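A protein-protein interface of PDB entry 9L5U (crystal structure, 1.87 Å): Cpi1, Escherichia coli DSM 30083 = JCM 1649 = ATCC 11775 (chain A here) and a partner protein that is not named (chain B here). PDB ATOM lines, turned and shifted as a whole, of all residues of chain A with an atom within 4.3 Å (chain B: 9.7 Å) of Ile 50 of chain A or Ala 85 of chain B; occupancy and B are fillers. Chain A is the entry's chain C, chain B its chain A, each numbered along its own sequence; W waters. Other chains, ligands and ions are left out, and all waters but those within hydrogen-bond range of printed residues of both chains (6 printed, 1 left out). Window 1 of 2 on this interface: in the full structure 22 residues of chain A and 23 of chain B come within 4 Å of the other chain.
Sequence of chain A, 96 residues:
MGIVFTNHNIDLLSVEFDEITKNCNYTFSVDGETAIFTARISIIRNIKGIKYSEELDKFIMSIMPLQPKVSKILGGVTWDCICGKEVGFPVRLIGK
O of Ala 85 of chain B is in hydrogen-bond range of N of Ile 50 of chain A (2.8 Å). N of Lys 48 of chain A lies within hydrogen-bond range of OG of Ser 90 of chain B (2.9 Å). The side-chain hydroxyl of Ser 87 of chain B sits at hydrogen-bond distance from the indole nitrogen of Trp 79 of chain A. O of Lys 48 of chain A sits at hydrogen-bond distance from N of Ser 87 of chain B (3.1 Å).
The backbone NH (N) of Asn 84 of chain B sits close to the side-chain sulfur (SD) of Met 67 of chain B (3.6 Å). The backbone carbonyl oxygen (O) of Arg 40 of chain A lies within hydrogen-bond range of the backbone NH (N) of Lys 51 of chain A, 2.8 Å away. N of Val 86 of chain B lies within hydrogen-bond range of O of Gly 150 of chain B (2.8 Å). ND1 of His 151 of chain B sits close to SD of Met 67 of chain B, 3.6 Å away. The side-chain amide oxygen of Asn 149 of chain B is in hydrogen-bond range of the backbone NH of His 151 of chain B.
Val 86 of chain B touches Lys 48 of chain A (CA to O, 3.4 Å). CA of Gly 49 of chain A touches O of Ala 85 of chain B (3.4 Å). Asn 84 of chain B touches Ile 50 of chain A. Lys 51 of chain A touches Asn 84 of chain B. Tyr 52 of chain A touches Met 67 of chain B. Tyr 52 of chain A touches Ala 85 of chain B (OH to CB, 3.6 Å). His 151 of chain B touches Tyr 52 of chain A (NE2 to CE2, 3.8 Å).
Of chain B, only Asn 84 and Ala 85 come within 4 Å of Ile 50 of chain A. No residue of chain B comes within 4 Å of Gly 75 of chain A. Of the printed residues of chain B, Trp 79 of chain A touches Ser 87. Printed residues of chain A within 4 Å of His 151 of chain B: Tyr 52 (3.8 Å). The nearest residue of chain B that does not touch Ile 50 of chain A is Met 67 of chain B (4.9 Å). The nearest printed residue of chain A that does not touch Asn 84 of chain B is Gly 49 of chain A (4.3 Å).
Of the 12 printed residues of chain A, 6 touch a printed residue of chain B. Printed residues of chain A that touch a printed residue of chain B: Lys 48, Gly 49, Ile 50, Lys 51, Tyr 52 and Trp 79. Hydrophobic or aromatic side chains of chain A that line the printed part of chain B: Ile 50, Tyr 52 and Trp 79. Along chain A the printed residues that touch a printed residue of chain B span positions 48 to 79. Among the printed residues, 11 pairs touch across the chains. Among the printed residues, no Asp or Glu carboxylate lies within 4 Å of a Lys or Arg side-chain nitrogen of the other chain.
Water W2 lies within hydrogen-bond range of the side-chain carboxylate (OE2) of Glu 82 of chain B (2.7 Å), the side-chain amide oxygen (OD1) of Asn 84 of chain B (2.7 Å), the backbone NH (N) of Gly 83 of chain B (2.9 Å) and the side-chain amino group (NZ) of Lys 51 of chain A (3.0 Å). Water W4 bridges O of Gly 83 of chain B and NZ of Lys 51 of chain A. Water W3 lies within hydrogen-bond range of OE2 of Glu 82 of chain B (2.9 Å) and NZ of Lys 51 of chain A (3.1 Å). Water W1 lies within hydrogen-bond range of NE1 of Trp 79 of chain A, O of Lys 48 of chain A, O of Ala 85 of chain B and N of Ser 87 of chain B.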
ATOM      1  N   TYR A  26     -14.804  14.325   1.988  1.00  0.00           N
ATOM      2  CA  TYR A  26     -14.087  15.232   2.869  1.00  0.00           C
ATOM      3  C   TYR A  26     -14.791  16.578   2.888  1.00  0.00           C
ATOM      4  O   TYR A  26     -15.121  17.114   1.827  1.00  0.00           O
ATOM      5  CB  TYR A  26     -12.679  15.455   2.365  1.00  0.00           C
ATOM      6  CG  TYR A  26     -11.781  14.261   2.330  1.00  0.00           C
ATOM      7  CD1 TYR A  26     -11.509  13.548   3.474  1.00  0.00           C
ATOM      8  CD2 TYR A  26     -11.161  13.880   1.151  1.00  0.00           C
ATOM      9  CE1 TYR A  26     -10.640  12.474   3.450  1.00  0.00           C
ATOM     10  CE2 TYR A  26     -10.282  12.819   1.115  1.00  0.00           C
ATOM     11  CZ  TYR A  26     -10.033  12.115   2.270  1.00  0.00           C
ATOM     12  OH  TYR A  26      -9.174  11.041   2.270  1.00  0.00           O
ATOM     13  N   ALA A  39     -13.033  11.439  -2.717  1.00  0.00           N
ATOM     14  CA  ALA A  39     -11.903  10.591  -3.044  1.00  0.00           C
ATOM     15  C   ALA A  39     -12.377   9.147  -2.958  1.00  0.00           C
ATOM     16  O   ALA A  39     -13.479   8.862  -2.480  1.00  0.00           O
ATOM     17  CB  ALA A  39     -10.738  10.805  -2.081  1.00  0.00           C
ATOM     18  N   ARG A  40     -11.513   8.226  -3.376  1.00  0.00           N
ATOM     19  CA  ARG A  40     -11.767   6.798  -3.233  1.00  0.00           C
ATOM     20  C   ARG A  40     -10.545   6.112  -2.654  1.00  0.00           C
ATOM     21  O   ARG A  40      -9.425   6.324  -3.128  1.00  0.00           O
ATOM     22  CB  ARG A  40     -12.125   6.166  -4.578  1.00  0.00           C
ATOM     23  CG  ARG A  40     -12.896   4.845  -4.450  1.00  0.00           C
ATOM     24  CD  ARG A  40     -12.355   3.784  -5.403  1.00  0.00           C
ATOM     25  NE  ARG A  40     -12.379   4.209  -6.804  1.00  0.00           N
ATOM     26  CZ  ARG A  40     -11.395   3.988  -7.677  1.00  0.00           C
ATOM     27  NH1 ARG A  40     -10.285   3.352  -7.300  1.00  0.00           N
ATOM     28  NH2 ARG A  40     -11.513   4.421  -8.928  1.00  0.00           N
ATOM     29  N   ILE A  41     -10.768   5.298  -1.640  1.00  0.00           N
ATOM     30  CA  ILE A  41      -9.703   4.549  -0.994  1.00  0.00           C
ATOM     31  C   ILE A  41      -9.327   3.372  -1.878  1.00  0.00           C
ATOM     32  O   ILE A  41     -10.197   2.675  -2.402  1.00  0.00           O
ATOM     33  CB  ILE A  41     -10.135   4.056   0.396  1.00  0.00           C
ATOM     34  CG1 ILE A  41     -10.592   5.221   1.265  1.00  0.00           C
ATOM     35  CG2 ILE A  41      -9.001   3.255   1.010  1.00  0.00           C
ATOM     36  CD1 ILE A  41      -9.597   6.312   1.376  1.00  0.00           C
ATOM     37  N   LYS A  48      -1.321   1.329   0.057  1.00  0.00           N
ATOM     38  CA  LYS A  48      -2.409   2.084   0.677  1.00  0.00           C
ATOM     39  C   LYS A  48      -2.501   3.442   0.004  1.00  0.00           C
ATOM     40  O   LYS A  48      -1.735   4.358   0.315  1.00  0.00           O
ATOM     41  CB  LYS A  48      -2.170   2.220   2.179  1.00  0.00           C
ATOM     42  CG  LYS A  48      -2.281   0.901   2.947  1.00  0.00           C
ATOM     43  CD  LYS A  48      -2.057   1.099   4.446  1.00  0.00           C
ATOM     44  CE  LYS A  48      -3.335   1.503   5.164  1.00  0.00           C
ATOM     45  NZ  LYS A  48      -3.061   2.501   6.240  1.00  0.00           N
ATOM     46  N   GLY A  49      -3.450   3.573  -0.912  1.00  0.00           N
ATOM     47  CA  GLY A  49      -3.586   4.785  -1.688  1.00  0.00           C
ATOM     48  C   GLY A  49      -4.922   5.469  -1.521  1.00  0.00           C
ATOM     49  O   GLY A  49      -5.921   4.833  -1.163  1.00  0.00           O
ATOM     50  N   ILE A  50      -4.945   6.773  -1.779  1.00  0.00           N
ATOM     51  CA  ILE A  50      -6.173   7.559  -1.836  1.00  0.00           C
ATOM     52  C   ILE A  50      -6.232   8.201  -3.214  1.00  0.00           C
ATOM     53  O   ILE A  50      -5.347   8.991  -3.582  1.00  0.00           O
ATOM     54  CB  ILE A  50      -6.233   8.625  -0.723  1.00  0.00           C
ATOM     55  CG1 ILE A  50      -6.102   7.959   0.654  1.00  0.00           C
ATOM     56  CG2 ILE A  50      -7.528   9.422  -0.808  1.00  0.00           C
ATOM     57  CD1 ILE A  50      -6.065   8.945   1.846  1.00  0.00           C
ATOM     58  N   LYS A  51      -7.269   7.868  -3.976  1.00  0.00           N
ATOM     59  CA  LYS A  51      -7.472   8.435  -5.304  1.00  0.00           C
ATOM     60  C   LYS A  51      -8.324   9.682  -5.144  1.00  0.00           C
ATOM     61  O   LYS A  51      -9.552   9.610  -5.042  1.00  0.00           O
ATOM     62  CB  LYS A  51      -8.119   7.428  -6.250  1.00  0.00           C
ATOM     63  CG  LYS A  51      -8.196   7.913  -7.699  1.00  0.00           C
ATOM     64  CD  LYS A  51      -8.925   6.875  -8.601  1.00  0.00           C
ATOM     65  CE  LYS A  51      -9.173   7.432 -10.009  1.00  0.00           C
ATOM     66  NZ  LYS A  51      -7.909   7.634 -10.782  1.00  0.00           N
ATOM     67  N   TYR A  52      -7.666  10.828  -5.087  1.00  0.00           N
ATOM     68  CA  TYR A  52      -8.392  12.082  -5.073  1.00  0.00           C
ATOM     69  C   TYR A  52      -9.195  12.223  -6.357  1.00  0.00           C
ATOM     70  O   TYR A  52      -8.733  11.851  -7.435  1.00  0.00           O
ATOM     71  CB  TYR A  52      -7.433  13.260  -4.983  1.00  0.00           C
ATOM     72  CG  TYR A  52      -6.567  13.363  -3.750  1.00  0.00           C
ATOM     73  CD1 TYR A  52      -6.903  12.735  -2.564  1.00  0.00           C
ATOM     74  CD2 TYR A  52      -5.392  14.119  -3.781  1.00  0.00           C
ATOM     75  CE1 TYR A  52      -6.086  12.856  -1.442  1.00  0.00           C
ATOM     76  CE2 TYR A  52      -4.565  14.231  -2.665  1.00  0.00           C
ATOM     77  CZ  TYR A  52      -4.926  13.609  -1.497  1.00  0.00           C
ATOM     78  OH  TYR A  52      -4.117  13.743  -0.375  1.00  0.00           O
ATOM     79  N   GLY A  75      -4.158  12.180   4.607  1.00  0.00           N
ATOM     80  CA  GLY A  75      -4.055  10.732   4.594  1.00  0.00           C
ATOM     81  C   GLY A  75      -3.995  10.134   5.984  1.00  0.00           C
ATOM     82  O   GLY A  75      -4.666   9.140   6.270  1.00  0.00           O
ATOM     83  N   THR A  78      -7.380  10.126   7.453  1.00  0.00           N
ATOM     84  CA  THR A  78      -8.276   9.218   6.740  1.00  0.00           C
ATOM     85  C   THR A  78      -8.088   7.778   7.206  1.00  0.00           C
ATOM     86  O   THR A  78      -9.061   7.098   7.558  1.00  0.00           O
ATOM     87  CB  THR A  78      -8.030   9.320   5.233  1.00  0.00           C
ATOM     88  OG1 THR A  78      -8.374  10.620   4.740  1.00  0.00           O
ATOM     89  CG2 THR A  78      -8.878   8.287   4.485  1.00  0.00           C
ATOM     90  N   TRP A  79      -6.836   7.295   7.211  1.00  0.00           N
ATOM     91  CA  TRP A  79      -6.565   5.916   7.624  1.00  0.00           C
ATOM     92  C   TRP A  79      -6.947   5.686   9.081  1.00  0.00           C
ATOM     93  O   TRP A  79      -7.456   4.609   9.411  1.00  0.00           O
ATOM     94  CB  TRP A  79      -5.091   5.551   7.324  1.00  0.00           C
ATOM     95  CG  TRP A  79      -4.834   5.540   5.824  1.00  0.00           C
ATOM     96  CD1 TRP A  79      -4.068   6.430   5.097  1.00  0.00           C
ATOM     97  CD2 TRP A  79      -5.386   4.625   4.864  1.00  0.00           C
ATOM     98  NE1 TRP A  79      -4.131   6.122   3.755  1.00  0.00           N
ATOM     99  CE2 TRP A  79      -4.923   5.020   3.586  1.00  0.00           C
ATOM    100  CE3 TRP A  79      -6.214   3.508   4.959  1.00  0.00           C
ATOM    101  CZ2 TRP A  79      -5.255   4.330   2.424  1.00  0.00           C
ATOM    102  CZ3 TRP A  79      -6.544   2.824   3.799  1.00  0.00           C
ATOM    103  CH2 TRP A  79      -6.063   3.238   2.552  1.00  0.00           C
ATOM    104  N   SER B  66       0.166  17.380 -12.152  1.00  0.00           N
ATOM    105  CA  SER B  66      -0.539  16.669 -11.097  1.00  0.00           C
ATOM    106  C   SER B  66      -0.530  15.161 -11.356  1.00  0.00           C
ATOM    107  O   SER B  66      -0.406  14.685 -12.496  1.00  0.00           O
ATOM    108  CB  SER B  66      -1.960  17.196 -10.930  1.00  0.00           C
ATOM    109  OG  SER B  66      -2.749  16.708 -11.995  1.00  0.00           O
ATOM    110  N   MET B  67      -0.652  14.393 -10.256  1.00  0.00           N
ATOM    111  CA  MET B  67      -0.645  12.940 -10.385  1.00  0.00           C
ATOM    112  C   MET B  67      -1.843  12.467 -11.197  1.00  0.00           C
ATOM    113  O   MET B  67      -1.749  11.489 -11.943  1.00  0.00           O
ATOM    114  CB  MET B  67      -0.643  12.271  -9.007  1.00  0.00           C
ATOM    115  CG  MET B  67      -1.891  12.522  -8.167  1.00  0.00           C
ATOM    116  SD  MET B  67      -1.596  11.853  -6.498  1.00  0.00           S
ATOM    117  CE  MET B  67      -2.933  12.680  -5.640  1.00  0.00           C
ATOM    118  N   THR B  68      -2.984  13.134 -11.036  1.00  0.00           N
ATOM    119  CA  THR B  68      -4.153  12.800 -11.842  1.00  0.00           C
ATOM    120  C   THR B  68      -3.846  12.960 -13.325  1.00  0.00           C
ATOM    121  O   THR B  68      -4.101  12.059 -14.132  1.00  0.00           O
ATOM    122  CB  THR B  68      -5.337  13.701 -11.439  1.00  0.00           C
ATOM    123  OG1 THR B  68      -5.816  13.257 -10.159  1.00  0.00           O
ATOM    124  CG2 THR B  68      -6.475  13.511 -12.465  1.00  0.00           C
ATOM    125  N   ALA B  71      -1.077  10.287 -14.475  1.00  0.00           N
ATOM    126  CA  ALA B  71      -1.583   8.922 -14.647  1.00  0.00           C
ATOM    127  C   ALA B  71      -2.557   8.855 -15.824  1.00  0.00           C
ATOM    128  O   ALA B  71      -2.550   7.882 -16.592  1.00  0.00           O
ATOM    129  CB  ALA B  71      -2.261   8.408 -13.364  1.00  0.00           C
ATOM    130  N   GLU B  82      -2.072   4.190 -11.910  1.00  0.00           N
ATOM    131  CA  GLU B  82      -2.745   4.889 -10.818  1.00  0.00           C
ATOM    132  C   GLU B  82      -1.999   6.177 -10.526  1.00  0.00           C
ATOM    133  O   GLU B  82      -0.776   6.231 -10.661  1.00  0.00           O
ATOM    134  CB  GLU B  82      -2.768   4.021  -9.544  1.00  0.00           C
ATOM    135  CG  GLU B  82      -3.435   2.640  -9.773  1.00  0.00           C
ATOM    136  CD  GLU B  82      -4.963   2.709  -9.987  1.00  0.00           C
ATOM    137  OE1 GLU B  82      -5.529   1.682 -10.385  1.00  0.00           O
ATOM    138  OE2 GLU B  82      -5.596   3.767  -9.769  1.00  0.00           O
ATOM    139  N   GLY B  83      -2.739   7.216 -10.148  1.00  0.00           N
ATOM    140  CA  GLY B  83      -2.153   8.466  -9.664  1.00  0.00           C
ATOM    141  C   GLY B  83      -2.831   8.810  -8.347  1.00  0.00           C
ATOM    142  O   GLY B  83      -3.911   9.417  -8.351  1.00  0.00           O
ATOM    143  N   ASN B  84      -2.215   8.391  -7.219  1.00  0.00           N
ATOM    144  CA  ASN B  84      -2.815   8.432  -5.884  1.00  0.00           C
ATOM    145  C   ASN B  84      -1.838   9.003  -4.854  1.00  0.00           C
ATOM    146  O   ASN B  84      -0.613   8.880  -4.995  1.00  0.00           O
ATOM    147  CB  ASN B  84      -3.242   7.014  -5.383  1.00  0.00           C
ATOM    148  CG  ASN B  84      -4.315   6.377  -6.260  1.00  0.00           C
ATOM    149  OD1 ASN B  84      -5.106   7.084  -6.892  1.00  0.00           O
ATOM    150  ND2 ASN B  84      -4.343   5.042  -6.302  1.00  0.00           N
ATOM    151  N   ALA B  85      -2.402   9.578  -3.785  1.00  0.00           N
ATOM    152  CA  ALA B  85      -1.624   9.909  -2.597  1.00  0.00           C
ATOM    153  C   ALA B  85      -1.460   8.629  -1.799  1.00  0.00           C
ATOM    154  O   ALA B  85      -2.454   7.995  -1.421  1.00  0.00           O
ATOM    155  CB  ALA B  85      -2.315  10.990  -1.757  1.00  0.00           C
ATOM    156  N   VAL B  86      -0.216   8.230  -1.562  1.00  0.00           N
ATOM    157  CA  VAL B  86       0.099   6.937  -0.975  1.00  0.00           C
ATOM    158  C   VAL B  86       0.783   7.146   0.371  1.00  0.00           C
ATOM    159  O   VAL B  86       1.581   8.073   0.525  1.00  0.00           O
ATOM    160  CB  VAL B  86       1.015   6.133  -1.918  1.00  0.00           C
ATOM    161  CG1 VAL B  86       1.475   4.855  -1.241  1.00  0.00           C
ATOM    162  CG2 VAL B  86       0.301   5.861  -3.262  1.00  0.00           C
ATOM    163  N   SER B  87       0.509   6.253   1.327  1.00  0.00           N
ATOM    164  CA  SER B  87       1.125   6.350   2.648  1.00  0.00           C
ATOM    165  C   SER B  87       2.626   6.118   2.579  1.00  0.00           C
ATOM    166  O   SER B  87       3.084   5.228   1.856  1.00  0.00           O
ATOM    167  CB  SER B  87       0.548   5.305   3.589  1.00  0.00           C
ATOM    168  OG  SER B  87      -0.815   5.562   3.828  1.00  0.00           O
ATOM    169  N   GLU B  88       3.373   6.862   3.410  1.00  0.00           N
ATOM    170  CA  GLU B  88       4.812   6.624   3.534  1.00  0.00           C
ATOM    171  C   GLU B  88       5.095   5.139   3.732  1.00  0.00           C
ATOM    172  O   GLU B  88       6.076   4.596   3.202  1.00  0.00           O
ATOM    173  CB  GLU B  88       5.386   7.431   4.704  1.00  0.00           C
ATOM    174  CG  GLU B  88       5.524   8.950   4.471  1.00  0.00           C
ATOM    175  CD  GLU B  88       6.129   9.693   5.664  1.00  0.00           C
ATOM    176  OE1 GLU B  88       6.064  10.941   5.700  1.00  0.00           O
ATOM    177  OE2 GLU B  88       6.680   9.039   6.576  1.00  0.00           O
ATOM    178  N   SER B  89       4.228   4.456   4.475  1.00  0.00           N
ATOM    179  CA  SER B  89       4.451   3.063   4.837  1.00  0.00           C
ATOM    180  C   SER B  89       4.344   2.106   3.654  1.00  0.00           C
ATOM    181  O   SER B  89       4.723   0.939   3.789  1.00  0.00           O
ATOM    182  CB  SER B  89       3.452   2.673   5.932  1.00  0.00           C
ATOM    183  OG  SER B  89       2.187   2.383   5.376  1.00  0.00           O
ATOM    184  N   SER B  90       3.836   2.550   2.503  1.00  0.00           N
ATOM    185  CA  SER B  90       3.720   1.684   1.332  1.00  0.00           C
ATOM    186  C   SER B  90       4.932   1.753   0.393  1.00  0.00           C
ATOM    187  O   SER B  90       4.843   1.243  -0.730  1.00  0.00           O
ATOM    188  CB  SER B  90       2.462   2.037   0.519  1.00  0.00           C
ATOM    189  OG  SER B  90       1.268   1.900   1.257  1.00  0.00           O
ATOM    190  N   LEU B  94       5.200  -0.243  -3.142  1.00  0.00           N
ATOM    191  CA  LEU B  94       5.265   0.435  -4.437  1.00  0.00           C
ATOM    192  C   LEU B  94       6.439  -0.096  -5.257  1.00  0.00           C
ATOM    193  O   LEU B  94       6.282  -0.460  -6.427  1.00  0.00           O
ATOM    194  CB  LEU B  94       5.380   1.953  -4.240  1.00  0.00           C
ATOM    195  CG  LEU B  94       4.095   2.711  -3.894  1.00  0.00           C
ATOM    196  CD1 LEU B  94       4.438   4.072  -3.299  1.00  0.00           C
ATOM    197  CD2 LEU B  94       3.218   2.854  -5.155  1.00  0.00           C
ATOM    198  N   TRP B 100       8.275   3.441 -10.323  1.00  0.00           N
ATOM    199  CA  TRP B 100       7.113   4.297 -10.127  1.00  0.00           C
ATOM    200  C   TRP B 100       7.607   5.725  -9.986  1.00  0.00           C
ATOM    201  O   TRP B 100       8.796   5.960  -9.775  1.00  0.00           O
ATOM    202  CB  TRP B 100       6.292   3.869  -8.885  1.00  0.00           C
ATOM    203  CG  TRP B 100       7.065   3.787  -7.590  1.00  0.00           C
ATOM    204  CD1 TRP B 100       7.926   2.797  -7.191  1.00  0.00           C
ATOM    205  CD2 TRP B 100       7.001   4.723  -6.507  1.00  0.00           C
ATOM    206  NE1 TRP B 100       8.422   3.091  -5.930  1.00  0.00           N
ATOM    207  CE2 TRP B 100       7.856   4.258  -5.493  1.00  0.00           C
ATOM    208  CE3 TRP B 100       6.295   5.916  -6.305  1.00  0.00           C
ATOM    209  CZ2 TRP B 100       8.042   4.952  -4.290  1.00  0.00           C
ATOM    210  CZ3 TRP B 100       6.477   6.606  -5.114  1.00  0.00           C
ATOM    211  CH2 TRP B 100       7.340   6.121  -4.119  1.00  0.00           C
ATOM    212  N   GLY B 101       6.694   6.682 -10.110  1.00  0.00           N
ATOM    213  CA  GLY B 101       7.035   8.098 -10.034  1.00  0.00           C
ATOM    214  C   GLY B 101       6.584   8.689  -8.700  1.00  0.00           C
ATOM    215  O   GLY B 101       5.460   8.444  -8.255  1.00  0.00           O
ATOM    216  N   MET B 103       6.392  12.307  -6.344  1.00  0.00           N
ATOM    217  CA  MET B 103       6.473  13.764  -6.321  1.00  0.00           C
ATOM    218  C   MET B 103       7.232  14.208  -5.078  1.00  0.00           C
ATOM    219  O   MET B 103       6.764  14.007  -3.955  1.00  0.00           O
ATOM    220  CB  MET B 103       5.086  14.415  -6.353  1.00  0.00           C
ATOM    221  CG  MET B 103       5.198  15.960  -6.557  1.00  0.00           C
ATOM    222  SD  MET B 103       3.620  16.828  -6.472  1.00  0.00           S
ATOM    223  CE  MET B 103       2.743  16.114  -7.864  1.00  0.00           C
ATOM    224  N   TRP B 114       8.896  15.730  -9.864  1.00  0.00           N
ATOM    225  CA  TRP B 114       8.743  14.293 -10.074  1.00  0.00           C
ATOM    226  C   TRP B 114      10.107  13.634 -10.247  1.00  0.00           C
ATOM    227  O   TRP B 114      10.949  14.128 -11.008  1.00  0.00           O
ATOM    228  CB  TRP B 114       7.889  14.027 -11.317  1.00  0.00           C
ATOM    229  CG  TRP B 114       6.421  14.291 -11.109  1.00  0.00           C
ATOM    230  CD1 TRP B 114       5.713  15.385 -11.501  1.00  0.00           C
ATOM    231  CD2 TRP B 114       5.486  13.416 -10.467  1.00  0.00           C
ATOM    232  NE1 TRP B 114       4.392  15.251 -11.139  1.00  0.00           N
ATOM    233  CE2 TRP B 114       4.230  14.052 -10.497  1.00  0.00           C
ATOM    234  CE3 TRP B 114       5.605  12.170  -9.845  1.00  0.00           C
ATOM    235  CZ2 TRP B 114       3.081  13.473  -9.943  1.00  0.00           C
ATOM    236  CZ3 TRP B 114       4.467  11.593  -9.291  1.00  0.00           C
ATOM    237  CH2 TRP B 114       3.221  12.249  -9.338  1.00  0.00           C
ATOM    238  N   TRP B 148       9.325  13.120  -0.248  1.00  0.00           N
ATOM    239  CA  TRP B 148       8.191  12.658  -1.042  1.00  0.00           C
ATOM    240  C   TRP B 148       6.884  13.071  -0.369  1.00  0.00           C
ATOM    241  O   TRP B 148       6.688  12.828   0.828  1.00  0.00           O
ATOM    242  CB  TRP B 148       8.284  11.142  -1.184  1.00  0.00           C
ATOM    243  CG  TRP B 148       7.098  10.412  -1.752  1.00  0.00           C
ATOM    244  CD1 TRP B 148       6.315  10.766  -2.832  1.00  0.00           C
ATOM    245  CD2 TRP B 148       6.613   9.149  -1.299  1.00  0.00           C
ATOM    246  NE1 TRP B 148       5.352   9.783  -3.051  1.00  0.00           N
ATOM    247  CE2 TRP B 148       5.516   8.794  -2.114  1.00  0.00           C
ATOM    248  CE3 TRP B 148       6.995   8.287  -0.257  1.00  0.00           C
ATOM    249  CZ2 TRP B 148       4.802   7.616  -1.923  1.00  0.00           C
ATOM    250  CZ3 TRP B 148       6.288   7.133  -0.062  1.00  0.00           C
ATOM    251  CH2 TRP B 148       5.198   6.799  -0.893  1.00  0.00           C
ATOM    252  N   ASN B 149       6.013  13.763  -1.103  1.00  0.00           N
ATOM    253  CA  ASN B 149       4.798  14.279  -0.472  1.00  0.00           C
ATOM    254  C   ASN B 149       3.657  13.267  -0.489  1.00  0.00           C
ATOM    255  O   ASN B 149       2.531  13.610  -0.116  1.00  0.00           O
ATOM    256  CB  ASN B 149       4.369  15.627  -1.113  1.00  0.00           C
ATOM    257  CG  ASN B 149       3.828  15.483  -2.537  1.00  0.00           C
ATOM    258  OD1 ASN B 149       3.743  14.391  -3.074  1.00  0.00           O
ATOM    259  ND2 ASN B 149       3.431  16.606  -3.138  1.00  0.00           N
ATOM    260  N   GLY B 150       3.925  12.021  -0.897  1.00  0.00           N
ATOM    261  CA  GLY B 150       2.893  11.001  -1.007  1.00  0.00           C
ATOM    262  C   GLY B 150       2.291  10.859  -2.404  1.00  0.00           C
ATOM    263  O   GLY B 150       1.764   9.789  -2.735  1.00  0.00           O
ATOM    264  N   HIS B 151       2.368  11.884  -3.241  1.00  0.00           N
ATOM    265  CA  HIS B 151       1.755  11.781  -4.566  1.00  0.00           C
ATOM    266  C   HIS B 151       2.597  10.869  -5.464  1.00  0.00           C
ATOM    267  O   HIS B 151       3.832  10.977  -5.518  1.00  0.00           O
ATOM    268  CB  HIS B 151       1.569  13.187  -5.159  1.00  0.00           C
ATOM    269  CG  HIS B 151       0.536  14.004  -4.425  1.00  0.00           C
ATOM    270  ND1 HIS B 151      -0.303  14.896  -5.056  1.00  0.00           N
ATOM    271  CD2 HIS B 151       0.203  14.046  -3.109  1.00  0.00           C
ATOM    272  CE1 HIS B 151      -1.113  15.449  -4.167  1.00  0.00           C
ATOM    273  NE2 HIS B 151      -0.820  14.956  -2.972  1.00  0.00           N
ATOM    274  N   SER B 152       1.933   9.942  -6.152  1.00  0.00           N
ATOM    275  CA  SER B 152       2.644   8.830  -6.763  1.00  0.00           C
ATOM    276  C   SER B 152       1.902   8.391  -8.014  1.00  0.00           C
ATOM    277  O   SER B 152       0.665   8.448  -8.072  1.00  0.00           O
ATOM    278  CB  SER B 152       2.757   7.628  -5.809  1.00  0.00           C
ATOM    279  OG  SER B 152       3.160   8.013  -4.495  1.00  0.00           O
ATOM    280  N   VAL B 153       2.679   7.949  -9.001  1.00  0.00           N
ATOM    281  CA  VAL B 153       2.173   7.360 -10.231  1.00  0.00           C
ATOM    282  C   VAL B 153       2.773   5.969 -10.325  1.00  0.00           C
ATOM    283  O   VAL B 153       4.009   5.815 -10.291  1.00  0.00           O
ATOM    284  CB  VAL B 153       2.539   8.232 -11.437  1.00  0.00           C
ATOM    285  CG1 VAL B 153       2.313   7.475 -12.703  1.00  0.00           C
ATOM    286  CG2 VAL B 153       1.653   9.496 -11.379  1.00  0.00           C
ATOM    287  N   TYR B 154       1.909   4.950 -10.355  1.00  0.00           N
ATOM    288  CA  TYR B 154       2.377   3.572 -10.292  1.00  0.00           C
ATOM    289  C   TYR B 154       1.398   2.653 -11.014  1.00  0.00           C
ATOM    290  O   TYR B 154       0.244   3.006 -11.263  1.00  0.00           O
ATOM    291  CB  TYR B 154       2.555   3.107  -8.839  1.00  0.00           C
ATOM    292  CG  TYR B 154       1.313   3.220  -7.954  1.00  0.00           C
ATOM    293  CD1 TYR B 154       0.914   4.445  -7.437  1.00  0.00           C
ATOM    294  CD2 TYR B 154       0.582   2.085  -7.591  1.00  0.00           C
ATOM    295  CE1 TYR B 154      -0.209   4.544  -6.588  1.00  0.00           C
ATOM    296  CE2 TYR B 154      -0.552   2.171  -6.740  1.00  0.00           C
ATOM    297  CZ  TYR B 154      -0.927   3.400  -6.236  1.00  0.00           C
ATOM    298  OH  TYR B 154      -2.049   3.519  -5.391  1.00  0.00           O
HETATM  299  O   HOH W   1      -2.755   6.857   1.367  1.00  0.00           O
HETATM  300  O   HOH W   2      -5.484   6.427  -9.516  1.00  0.00           O
HETATM  301  O   HOH W   3      -7.884   4.565 -11.271  1.00  0.00           O
HETATM  302  O   HOH W   4      -5.854   9.650 -10.375  1.00  0.00           O
HETATM  303  O   HOH W   5      -6.845   3.630  -7.394  1.00  0.00           O
HETATM  304  O   HOH W   6      -5.624  11.091  -7.017  1.00  0.00           O
